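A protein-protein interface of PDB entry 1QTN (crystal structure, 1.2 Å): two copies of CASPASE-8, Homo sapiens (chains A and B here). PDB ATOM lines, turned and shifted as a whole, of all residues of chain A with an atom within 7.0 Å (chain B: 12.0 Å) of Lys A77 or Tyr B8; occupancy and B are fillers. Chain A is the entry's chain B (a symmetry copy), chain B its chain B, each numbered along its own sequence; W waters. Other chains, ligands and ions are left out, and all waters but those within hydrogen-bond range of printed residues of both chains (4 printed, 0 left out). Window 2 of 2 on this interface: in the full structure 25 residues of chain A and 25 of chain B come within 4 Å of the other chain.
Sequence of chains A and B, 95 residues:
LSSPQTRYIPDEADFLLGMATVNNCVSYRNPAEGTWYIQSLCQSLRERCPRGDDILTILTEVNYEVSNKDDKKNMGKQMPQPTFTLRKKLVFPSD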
ATOM      1  N   THR A  21      -6.673 -14.778  -0.524  1.00  0.00           N
ATOM      2  CA  THR A  21      -7.561 -15.898  -0.768  1.00  0.00           C
ATOM      3  C   THR A  21      -7.302 -17.019   0.244  1.00  0.00           C
ATOM      4  O   THR A  21      -6.145 -17.249   0.632  1.00  0.00           O
ATOM      5  CB  THR A  21      -7.398 -16.440  -2.187  1.00  0.00           C
ATOM      6  OG1 THR A  21      -8.235 -17.590  -2.402  1.00  0.00           O
ATOM      7  CG2 THR A  21      -5.980 -16.832  -2.512  1.00  0.00           C
ATOM      8  N   CYS A  25      -7.294 -21.731  -4.122  1.00  0.00           N
ATOM      9  CA  CYS A  25      -8.009 -20.873  -5.032  1.00  0.00           C
ATOM     10  C   CYS A  25      -7.209 -19.720  -5.581  1.00  0.00           C
ATOM     11  O   CYS A  25      -6.245 -19.242  -4.989  1.00  0.00           O
ATOM     12  CB  CYS A  25      -9.328 -20.385  -4.445  1.00  0.00           C
ATOM     13  SG  CYS A  25     -10.452 -21.731  -3.992  1.00  0.00           S
ATOM     14  N   VAL A  26      -7.696 -19.178  -6.705  1.00  0.00           N
ATOM     15  CA  VAL A  26      -7.135 -17.998  -7.321  1.00  0.00           C
ATOM     16  C   VAL A  26      -7.516 -16.744  -6.552  1.00  0.00           C
ATOM     17  O   VAL A  26      -8.499 -16.705  -5.801  1.00  0.00           O
ATOM     18  CB  VAL A  26      -7.593 -17.860  -8.785  1.00  0.00           C
ATOM     19  CG1 VAL A  26      -7.170 -19.046  -9.612  1.00  0.00           C
ATOM     20  CG2 VAL A  26      -9.079 -17.597  -8.908  1.00  0.00           C
ATOM     21  N   SER A  27      -6.759 -15.688  -6.794  1.00  0.00           N
ATOM     22  CA  SER A  27      -7.197 -14.345  -6.481  1.00  0.00           C
ATOM     23  C   SER A  27      -7.103 -13.501  -7.773  1.00  0.00           C
ATOM     24  O   SER A  27      -6.387 -13.905  -8.702  1.00  0.00           O
ATOM     25  CB  SER A  27      -6.464 -13.675  -5.352  1.00  0.00           C
ATOM     26  OG  SER A  27      -5.092 -13.573  -5.565  1.00  0.00           O
ATOM     27  N   TYR A  28      -7.811 -12.392  -7.787  1.00  0.00           N
ATOM     28  CA  TYR A  28      -8.024 -11.635  -8.980  1.00  0.00           C
ATOM     29  C   TYR A  28      -7.241 -10.342  -9.064  1.00  0.00           C
ATOM     30  O   TYR A  28      -7.084  -9.606  -8.084  1.00  0.00           O
ATOM     31  CB  TYR A  28      -9.487 -11.382  -9.218  1.00  0.00           C
ATOM     32  CG  TYR A  28     -10.277 -12.630  -9.567  1.00  0.00           C
ATOM     33  CD1 TYR A  28     -10.217 -13.111 -10.872  1.00  0.00           C
ATOM     34  CD2 TYR A  28     -11.028 -13.302  -8.641  1.00  0.00           C
ATOM     35  CE1 TYR A  28     -10.934 -14.225 -11.241  1.00  0.00           C
ATOM     36  CE2 TYR A  28     -11.794 -14.393  -9.006  1.00  0.00           C
ATOM     37  CZ  TYR A  28     -11.727 -14.850 -10.303  1.00  0.00           C
ATOM     38  OH  TYR A  28     -12.460 -15.948 -10.687  1.00  0.00           O
ATOM     39  N   TRP A  36      -8.249  -7.112  -6.521  1.00  0.00           N
ATOM     40  CA  TRP A  36      -9.440  -6.939  -5.689  1.00  0.00           C
ATOM     41  C   TRP A  36      -9.018  -6.740  -4.218  1.00  0.00           C
ATOM     42  O   TRP A  36      -9.516  -5.854  -3.551  1.00  0.00           O
ATOM     43  CB  TRP A  36     -10.306  -8.201  -5.792  1.00  0.00           C
ATOM     44  CG  TRP A  36     -11.025  -8.384  -7.083  1.00  0.00           C
ATOM     45  CD1 TRP A  36     -10.969  -7.607  -8.202  1.00  0.00           C
ATOM     46  CD2 TRP A  36     -12.025  -9.400  -7.357  1.00  0.00           C
ATOM     47  NE1 TRP A  36     -11.850  -8.095  -9.161  1.00  0.00           N
ATOM     48  CE2 TRP A  36     -12.480  -9.183  -8.683  1.00  0.00           C
ATOM     49  CE3 TRP A  36     -12.519 -10.462  -6.627  1.00  0.00           C
ATOM     50  CZ2 TRP A  36     -13.446 -10.040  -9.240  1.00  0.00           C
ATOM     51  CZ3 TRP A  36     -13.478 -11.295  -7.186  1.00  0.00           C
ATOM     52  CH2 TRP A  36     -13.905 -11.069  -8.498  1.00  0.00           C
ATOM     53  N   VAL A  66     -14.777  -7.734  -0.784  1.00  0.00           N
ATOM     54  CA  VAL A  66     -14.279  -8.664  -1.775  1.00  0.00           C
ATOM     55  C   VAL A  66     -15.266  -9.781  -2.048  1.00  0.00           C
ATOM     56  O   VAL A  66     -15.441 -10.195  -3.203  1.00  0.00           O
ATOM     57  CB  VAL A  66     -12.870  -9.188  -1.431  1.00  0.00           C
ATOM     58  CG1 VAL A  66     -12.383 -10.201  -2.448  1.00  0.00           C
ATOM     59  CG2 VAL A  66     -11.879  -8.013  -1.381  1.00  0.00           C
ATOM     60  N   SER A  67     -16.013 -10.217  -1.034  1.00  0.00           N
ATOM     61  CA  SER A  67     -17.042 -11.223  -1.199  1.00  0.00           C
ATOM     62  C   SER A  67     -18.162 -10.780  -2.122  1.00  0.00           C
ATOM     63  O   SER A  67     -18.883 -11.684  -2.625  1.00  0.00           O
ATOM     64  CB  SER A  67     -17.632 -11.620   0.164  1.00  0.00           C
ATOM     65  OG  SER A  67     -16.723 -12.422   0.902  1.00  0.00           O
ATOM     66  N   ASN A  68     -18.351  -9.509  -2.329  1.00  0.00           N
ATOM     67  CA  ASN A  68     -19.425  -9.033  -3.234  1.00  0.00           C
ATOM     68  C   ASN A  68     -18.975  -8.922  -4.652  1.00  0.00           C
ATOM     69  O   ASN A  68     -19.826  -8.765  -5.567  1.00  0.00           O
ATOM     70  CB  ASN A  68     -19.994  -7.717  -2.723  1.00  0.00           C
ATOM     71  CG  ASN A  68     -20.743  -7.915  -1.411  1.00  0.00           C
ATOM     72  OD1 ASN A  68     -21.264  -8.994  -1.142  1.00  0.00           O
ATOM     73  ND2 ASN A  68     -20.749  -6.882  -0.586  1.00  0.00           N
ATOM     74  N   LYS A  69     -17.708  -9.013  -4.966  1.00  0.00           N
ATOM     75  CA  LYS A  69     -17.195  -8.944  -6.323  1.00  0.00           C
ATOM     76  C   LYS A  69     -17.340 -10.262  -7.046  1.00  0.00           C
ATOM     77  O   LYS A  69     -17.386 -11.346  -6.442  1.00  0.00           O
ATOM     78  CB  LYS A  69     -15.699  -8.558  -6.302  1.00  0.00           C
ATOM     79  CG  LYS A  69     -15.477  -7.193  -5.640  1.00  0.00           C
ATOM     80  CD  LYS A  69     -13.988  -6.874  -5.629  1.00  0.00           C
ATOM     81  CE  LYS A  69     -13.645  -5.743  -4.682  1.00  0.00           C
ATOM     82  NZ  LYS A  69     -14.305  -4.465  -5.093  1.00  0.00           N
ATOM     83  N   ASP A  70     -17.419 -10.227  -8.373  1.00  0.00           N
ATOM     84  CA  ASP A  70     -17.453 -11.483  -9.097  1.00  0.00           C
ATOM     85  C   ASP A  70     -16.748 -11.422 -10.434  1.00  0.00           C
ATOM     86  O   ASP A  70     -16.551 -10.324 -11.002  1.00  0.00           O
ATOM     87  CB  ASP A  70     -18.850 -12.045  -9.242  1.00  0.00           C
ATOM     88  CG  ASP A  70     -19.817 -11.042  -9.769  1.00  0.00           C
ATOM     89  OD1 ASP A  70     -19.406 -10.267 -10.688  1.00  0.00           O
ATOM     90  OD2 ASP A  70     -20.950 -10.923  -9.257  1.00  0.00           O
ATOM     91  N   ASP A  71     -16.379 -12.585 -10.880  1.00  0.00           N
ATOM     92  CA  ASP A  71     -15.792 -12.821 -12.216  1.00  0.00           C
ATOM     93  C   ASP A  71     -16.901 -13.490 -13.060  1.00  0.00           C
ATOM     94  O   ASP A  71     -17.141 -14.680 -12.887  1.00  0.00           O
ATOM     95  CB  ASP A  71     -14.610 -13.759 -12.032  1.00  0.00           C
ATOM     96  CG  ASP A  71     -14.107 -14.435 -13.270  1.00  0.00           C
ATOM     97  OD1 ASP A  71     -14.516 -13.990 -14.385  1.00  0.00           O
ATOM     98  OD2 ASP A  71     -13.317 -15.376 -13.157  1.00  0.00           O
ATOM     99  N   ASN A  74     -15.915 -16.752 -15.529  1.00  0.00           N
ATOM    100  CA  ASN A  74     -15.781 -18.085 -15.003  1.00  0.00           C
ATOM    101  C   ASN A  74     -16.735 -18.341 -13.812  1.00  0.00           C
ATOM    102  O   ASN A  74     -16.606 -19.409 -13.201  1.00  0.00           O
ATOM    103  CB  ASN A  74     -14.355 -18.330 -14.498  1.00  0.00           C
ATOM    104  CG  ASN A  74     -13.355 -18.157 -15.639  1.00  0.00           C
ATOM    105  OD1 ASN A  74     -13.399 -18.904 -16.609  1.00  0.00           O
ATOM    106  ND2 ASN A  74     -12.533 -17.127 -15.526  1.00  0.00           N
ATOM    107  N   MET A  75     -17.599 -17.434 -13.534  1.00  0.00           N
ATOM    108  CA  MET A  75     -18.501 -17.537 -12.368  1.00  0.00           C
ATOM    109  C   MET A  75     -17.678 -17.749 -11.098  1.00  0.00           C
ATOM    110  O   MET A  75     -17.869 -18.724 -10.375  1.00  0.00           O
ATOM    111  CB  MET A  75     -19.471 -18.712 -12.582  1.00  0.00           C
ATOM    112  CG  MET A  75     -20.342 -18.499 -13.822  1.00  0.00           C
ATOM    113  SD  MET A  75     -21.124 -16.870 -13.812  1.00  0.00           S
ATOM    114  CE  MET A  75     -21.558 -16.670 -15.534  1.00  0.00           C
ATOM    115  N   GLY A  76     -16.657 -16.916 -10.938  1.00  0.00           N
ATOM    116  CA  GLY A  76     -15.753 -16.993  -9.819  1.00  0.00           C
ATOM    117  C   GLY A  76     -15.970 -15.914  -8.784  1.00  0.00           C
ATOM    118  O   GLY A  76     -16.406 -14.808  -9.019  1.00  0.00           O
ATOM    119  N   LYS A  77     -15.600 -16.302  -7.551  1.00  0.00           N
ATOM    120  CA  LYS A  77     -15.642 -15.408  -6.396  1.00  0.00           C
ATOM    121  C   LYS A  77     -14.236 -15.433  -5.764  1.00  0.00           C
ATOM    122  O   LYS A  77     -13.358 -16.165  -6.217  1.00  0.00           O
ATOM    123  CB  LYS A  77     -16.656 -15.934  -5.373  1.00  0.00           C
ATOM    124  CG  LYS A  77     -18.076 -15.984  -5.883  1.00  0.00           C
ATOM    125  CD  LYS A  77     -18.690 -14.651  -6.182  1.00  0.00           C
ATOM    126  CE  LYS A  77     -19.152 -13.932  -4.914  1.00  0.00           C
ATOM    127  NZ  LYS A  77     -19.621 -12.550  -5.188  1.00  0.00           N
ATOM    128  N   GLN A  78     -14.045 -14.624  -4.733  1.00  0.00           N
ATOM    129  CA  GLN A  78     -12.767 -14.593  -4.019  1.00  0.00           C
ATOM    130  C   GLN A  78     -13.054 -14.342  -2.516  1.00  0.00           C
ATOM    131  O   GLN A  78     -13.797 -13.449  -2.203  1.00  0.00           O
ATOM    132  CB  GLN A  78     -11.878 -13.469  -4.545  1.00  0.00           C
ATOM    133  CG  GLN A  78     -10.489 -13.479  -3.878  1.00  0.00           C
ATOM    134  CD  GLN A  78      -9.612 -12.403  -4.447  1.00  0.00           C
ATOM    135  OE1 GLN A  78      -9.657 -12.074  -5.637  1.00  0.00           O
ATOM    136  NE2 GLN A  78      -8.800 -11.782  -3.601  1.00  0.00           N
ATOM    137  N   MET A  79     -12.441 -15.193  -1.704  1.00  0.00           N
ATOM    138  CA  MET A  79     -12.617 -15.104  -0.248  1.00  0.00           C
ATOM    139  C   MET A  79     -11.272 -14.869   0.445  1.00  0.00           C
ATOM    140  O   MET A  79     -10.500 -15.797   0.619  1.00  0.00           O
ATOM    141  CB  MET A  79     -13.206 -16.425   0.272  1.00  0.00           C
ATOM    142  CG  MET A  79     -13.604 -16.333   1.761  1.00  0.00           C
ATOM    143  SD  MET A  79     -14.980 -15.229   2.043  1.00  0.00           S
ATOM    144  CE  MET A  79     -14.267 -13.841   2.884  1.00  0.00           C
ATOM    145  N   THR B   6     -30.256 -13.059  -7.672  1.00  0.00           N
ATOM    146  CA  THR B   6     -30.009 -12.873  -6.237  1.00  0.00           C
ATOM    147  C   THR B   6     -28.580 -12.428  -5.994  1.00  0.00           C
ATOM    148  O   THR B   6     -27.833 -12.239  -6.968  1.00  0.00           O
ATOM    149  CB  THR B   6     -30.417 -14.029  -5.373  1.00  0.00           C
ATOM    150  OG1 THR B   6     -29.462 -15.079  -5.322  1.00  0.00           O
ATOM    151  CG2 THR B   6     -31.755 -14.641  -5.736  1.00  0.00           C
ATOM    152  N   ARG B   7     -28.157 -12.245  -4.735  1.00  0.00           N
ATOM    153  CA  ARG B   7     -26.728 -11.905  -4.524  1.00  0.00           C
ATOM    154  C   ARG B   7     -25.954 -13.137  -4.108  1.00  0.00           C
ATOM    155  O   ARG B   7     -26.486 -14.016  -3.433  1.00  0.00           O
ATOM    156  CB  ARG B   7     -26.579 -10.803  -3.485  1.00  0.00           C
ATOM    157  CG  ARG B   7     -27.280  -9.506  -3.875  1.00  0.00           C
ATOM    158  CD  ARG B   7     -26.319  -8.443  -4.351  1.00  0.00           C
ATOM    159  NE  ARG B   7     -26.876  -7.652  -5.437  1.00  0.00           N
ATOM    160  CZ  ARG B   7     -26.179  -6.976  -6.335  1.00  0.00           C
ATOM    161  NH1 ARG B   7     -26.808  -6.298  -7.291  1.00  0.00           N
ATOM    162  NH2 ARG B   7     -24.855  -6.951  -6.289  1.00  0.00           N
ATOM    163  N   TYR B   8     -24.670 -13.165  -4.491  1.00  0.00           N
ATOM    164  CA  TYR B   8     -23.796 -14.286  -4.230  1.00  0.00           C
ATOM    165  C   TYR B   8     -22.559 -13.863  -3.413  1.00  0.00           C
ATOM    166  O   TYR B   8     -22.015 -12.799  -3.609  1.00  0.00           O
ATOM    167  CB  TYR B   8     -23.330 -14.960  -5.531  1.00  0.00           C
ATOM    168  CG  TYR B   8     -24.528 -15.577  -6.272  1.00  0.00           C
ATOM    169  CD1 TYR B   8     -25.369 -14.768  -7.025  1.00  0.00           C
ATOM    170  CD2 TYR B   8     -24.809 -16.911  -6.177  1.00  0.00           C
ATOM    171  CE1 TYR B   8     -26.440 -15.339  -7.741  1.00  0.00           C
ATOM    172  CE2 TYR B   8     -25.907 -17.481  -6.822  1.00  0.00           C
ATOM    173  CZ  TYR B   8     -26.740 -16.655  -7.536  1.00  0.00           C
ATOM    174  OH  TYR B   8     -27.850 -17.228  -8.192  1.00  0.00           O
ATOM    175  N   ILE B   9     -22.175 -14.757  -2.501  1.00  0.00           N
ATOM    176  CA  ILE B   9     -20.918 -14.602  -1.728  1.00  0.00           C
ATOM    177  C   ILE B   9     -20.110 -15.866  -1.888  1.00  0.00           C
ATOM    178  O   ILE B   9     -20.577 -16.873  -2.453  1.00  0.00           O
ATOM    179  CB  ILE B   9     -21.231 -14.319  -0.246  1.00  0.00           C
ATOM    180  CG1 ILE B   9     -22.001 -15.434   0.433  1.00  0.00           C
ATOM    181  CG2 ILE B   9     -21.914 -12.962  -0.136  1.00  0.00           C
ATOM    182  CD1 ILE B   9     -22.214 -15.234   1.938  1.00  0.00           C
ATOM    183  N   PRO B  10     -18.854 -15.913  -1.454  1.00  0.00           N
ATOM    184  CA  PRO B  10     -18.054 -17.104  -1.607  1.00  0.00           C
ATOM    185  C   PRO B  10     -18.526 -18.305  -0.803  1.00  0.00           C
ATOM    186  O   PRO B  10     -19.024 -18.157   0.322  1.00  0.00           O
ATOM    187  CB  PRO B  10     -16.658 -16.672  -1.127  1.00  0.00           C
ATOM    188  CG  PRO B  10     -16.661 -15.164  -1.365  1.00  0.00           C
ATOM    189  CD  PRO B  10     -18.051 -14.748  -0.985  1.00  0.00           C
ATOM    190  N   ASP B  11     -18.379 -19.501  -1.361  1.00  0.00           N
ATOM    191  CA  ASP B  11     -18.679 -20.754  -0.717  1.00  0.00           C
ATOM    192  C   ASP B  11     -18.068 -20.850   0.682  1.00  0.00           C
ATOM    193  O   ASP B  11     -18.696 -21.424   1.576  1.00  0.00           O
ATOM    194  CB  ASP B  11     -18.118 -21.882  -1.617  1.00  0.00           C
ATOM    195  CG  ASP B  11     -18.519 -23.264  -1.143  1.00  0.00           C
ATOM    196  OD1 ASP B  11     -19.655 -23.445  -0.725  1.00  0.00           O
ATOM    197  OD2 ASP B  11     -17.668 -24.176  -1.275  1.00  0.00           O
ATOM    198  N   GLU B  12     -16.901 -20.319   0.903  1.00  0.00           N
ATOM    199  CA  GLU B  12     -16.098 -20.441   2.098  1.00  0.00           C
ATOM    200  C   GLU B  12     -16.202 -19.227   2.979  1.00  0.00           C
ATOM    201  O   GLU B  12     -15.382 -19.065   3.902  1.00  0.00           O
ATOM    202  CB  GLU B  12     -14.678 -20.866   1.804  1.00  0.00           C
ATOM    203  CG  GLU B  12     -14.557 -22.269   1.244  1.00  0.00           C
ATOM    204  CD  GLU B  12     -13.160 -22.685   0.887  1.00  0.00           C
ATOM    205  OE1 GLU B  12     -12.215 -22.503   1.681  1.00  0.00           O
ATOM    206  OE2 GLU B  12     -12.971 -23.099  -0.299  1.00  0.00           O
ATOM    207  N   ALA B  13     -17.193 -18.383   2.780  1.00  0.00           N
ATOM    208  CA  ALA B  13     -17.412 -17.230   3.625  1.00  0.00           C
ATOM    209  C   ALA B  13     -17.918 -17.620   4.999  1.00  0.00           C
ATOM    210  O   ALA B  13     -18.487 -18.692   5.241  1.00  0.00           O
ATOM    211  CB  ALA B  13     -18.429 -16.283   2.961  1.00  0.00           C
ATOM    212  N   ASP B  14     -17.742 -16.690   5.953  1.00  0.00           N
ATOM    213  CA  ASP B  14     -18.396 -16.776   7.231  1.00  0.00           C
ATOM    214  C   ASP B  14     -17.911 -17.829   8.159  1.00  0.00           C
ATOM    215  O   ASP B  14     -18.659 -18.303   9.033  1.00  0.00           O
ATOM    216  CB  ASP B  14     -19.928 -16.794   7.098  1.00  0.00           C
ATOM    217  CG  ASP B  14     -20.438 -15.729   6.135  1.00  0.00           C
ATOM    218  OD1 ASP B  14     -20.089 -14.547   6.295  1.00  0.00           O
ATOM    219  OD2 ASP B  14     -21.187 -16.088   5.186  1.00  0.00           O
ATOM    220  N   THR B  85     -12.873 -16.039   7.772  1.00  0.00           N
ATOM    221  CA  THR B  85     -13.474 -15.497   6.560  1.00  0.00           C
ATOM    222  C   THR B  85     -14.767 -14.775   6.898  1.00  0.00           C
ATOM    223  O   THR B  85     -15.618 -14.495   6.033  1.00  0.00           O
ATOM    224  CB  THR B  85     -13.656 -16.531   5.456  1.00  0.00           C
ATOM    225  OG1 THR B  85     -14.496 -17.553   5.957  1.00  0.00           O
ATOM    226  CG2 THR B  85     -12.353 -17.171   5.040  1.00  0.00           C
ATOM    227  N   ARG B  87     -17.332 -11.882   7.516  1.00  0.00           N
ATOM    228  CA  ARG B  87     -17.620 -10.682   6.739  1.00  0.00           C
ATOM    229  C   ARG B  87     -18.359  -9.636   7.566  1.00  0.00           C
ATOM    230  O   ARG B  87     -18.553  -8.520   7.063  1.00  0.00           O
ATOM    231  CB  ARG B  87     -18.476 -11.017   5.525  1.00  0.00           C
ATOM    232  CG  ARG B  87     -17.911 -11.945   4.515  1.00  0.00           C
ATOM    233  CD  ARG B  87     -18.905 -12.359   3.436  1.00  0.00           C
ATOM    234  NE  ARG B  87     -20.114 -12.867   4.011  1.00  0.00           N
ATOM    235  CZ  ARG B  87     -21.325 -12.337   4.038  1.00  0.00           C
ATOM    236  NH1 ARG B  87     -21.648 -11.221   3.406  1.00  0.00           N
ATOM    237  NH2 ARG B  87     -22.250 -12.927   4.757  1.00  0.00           N
ATOM    238  N   LYS B  88     -18.720  -9.955   8.787  1.00  0.00           N
ATOM    239  CA  LYS B  88     -19.386  -9.042   9.703  1.00  0.00           C
ATOM    240  C   LYS B  88     -18.814  -9.270  11.117  1.00  0.00           C
ATOM    241  O   LYS B  88     -18.135 -10.279  11.318  1.00  0.00           O
ATOM    242  CB  LYS B  88     -20.904  -9.350   9.730  1.00  0.00           C
ATOM    243  CG  LYS B  88     -21.570  -9.328   8.357  1.00  0.00           C
ATOM    244  CD  LYS B  88     -23.058  -9.615   8.428  1.00  0.00           C
ATOM    245  CE  LYS B  88     -23.716  -9.489   7.062  1.00  0.00           C
ATOM    246  NZ  LYS B  88     -25.151  -9.930   7.116  1.00  0.00           N
HETATM  247  O   HOH W   1     -10.992 -24.411  -1.546  1.00  0.00           O
HETATM  248  O   HOH W   2     -20.268  -9.765   1.320  1.00  0.00           O
HETATM  249  O   HOH W   3     -22.652  -8.747  -5.288  1.00  0.00           O
HETATM  250  O   HOH W   4     -22.953 -10.247  -2.870  1.00  0.00           O
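Thr A21 touches none of the printed residues of chain B.
Cys A25 touches none of the printed residues of chain B.
No residue of chain B comes within 4 Å of Val A26.
Printed residues of chain B within 4 Å of Ser A67: Tyr B8 (3.5 Å), Ile B9 (3.7 Å), Pro B10 (3.3 Å) and Arg B87 (3.3 Å).
No residue of chain B comes within 4 Å of Asp A70.
Of the printed residues of chain B, Lys A77 touches Tyr B8, Ile B9 and Pro B10.
Tyr B8 touches two residues of chain A.
Of the printed residues of chain A, Ile B9 touches Ser A67 and Lys A77.
Of the printed residues of chain A, Pro B10 touches Ser A67 (3.3 Å), Lys A77 (3.998 Å), Gln A78 (3.4 Å) and Met A79 (3.7 Å).
Of the printed residues of chain A, Glu B12 touches Met A79.
Printed residues of chain A within 4 Å of Arg B87: Ser A67 (3.3 Å).
The nearest residue of chain A that does not touch Tyr B8 is Asn A68 (4.6 Å).
Water W1 lies within hydrogen-bond range of the side-chain carboxylate of Glu B12 and the side-chain sulfur of Cys A25.
Water W4 lies within hydrogen-bond range of the side-chain amide oxygen (OD1) of Asn A68 and the backbone carbonyl oxygen (O) of Tyr B8.
Water W2 bridges OD1 of Asn A68 (2.8 Å) and NH1 of Arg B87 (2.9 Å).
Water W3 bridges the backbone carbonyl oxygen of Asn A68 (2.8 Å) and the guanidinium group of Arg B7 (3.0 Å).
Hydrophobic or aromatic side chains of chain B within 4 Å of the printed part of chain A: Pro B10 and Ala B13.
Hydrophobic or aromatic side chains of chain A within 4 Å of the printed part of chain B: Met A79.
Among the printed residues, 12 pairs touch across the chains.
Among the printed residues, no Asp or Glu carboxylate lies within 4 Å of a Lys or Arg side-chain nitrogen of the other chain.
Among the printed residues, merely in contact across the chains: Ser A67 with Pro B10 (3.3 Å), Ser A67 with Arg B87 (3.3 Å), Gln A78 with Pro B10 (3.4 Å), Met A79 with Thr B85 (3.5 Å), Met A79 with Ala B13 (3.5 Å), Ser A67 with Ile B9 (3.7 Å), Lys A77 with Ile B9 (3.7 Å), Met A79 with Pro B10 (3.7 Å), Met A79 with Glu B12 (3.9 Å) and Lys A77 with Pro B10 (3.998 Å).
O of Tyr B8 is in hydrogen-bond range of NZ of Lys A77 (2.9 Å).
The backbone carbonyl oxygen (O) of Ser A67 lies close to the backbone carbonyl oxygen (O) of Tyr B8.
No position is printed for both chains.
Of the 12 pairs that touch across the chains among the printed residues, none has its exchanged pair printed and touching as well.
The side-chain hydroxyl of Thr B85 is in hydrogen-bond range of the backbone carbonyl oxygen of Glu B12.
The backbone NH (N) of Asp B14 sits at hydrogen-bond distance from the backbone carbonyl oxygen (O) of Thr B85 (3.1 Å).
The guanidinium group (NE) of Arg B87 lies within salt-bridge range of the side-chain carboxylate (OD1) of Asp B14 (2.8 Å).
N of Tyr A28 lies within hydrogen-bond range of OE1 of Gln A78 (2.9 Å).
The side-chain amino group (NZ) of Lys A77 lies within hydrogen-bond range of the backbone carbonyl oxygen (O) of Ser A67 (2.8 Å).
SD of Met A79 lies close to OG of Ser A67, at 3.5 Å.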
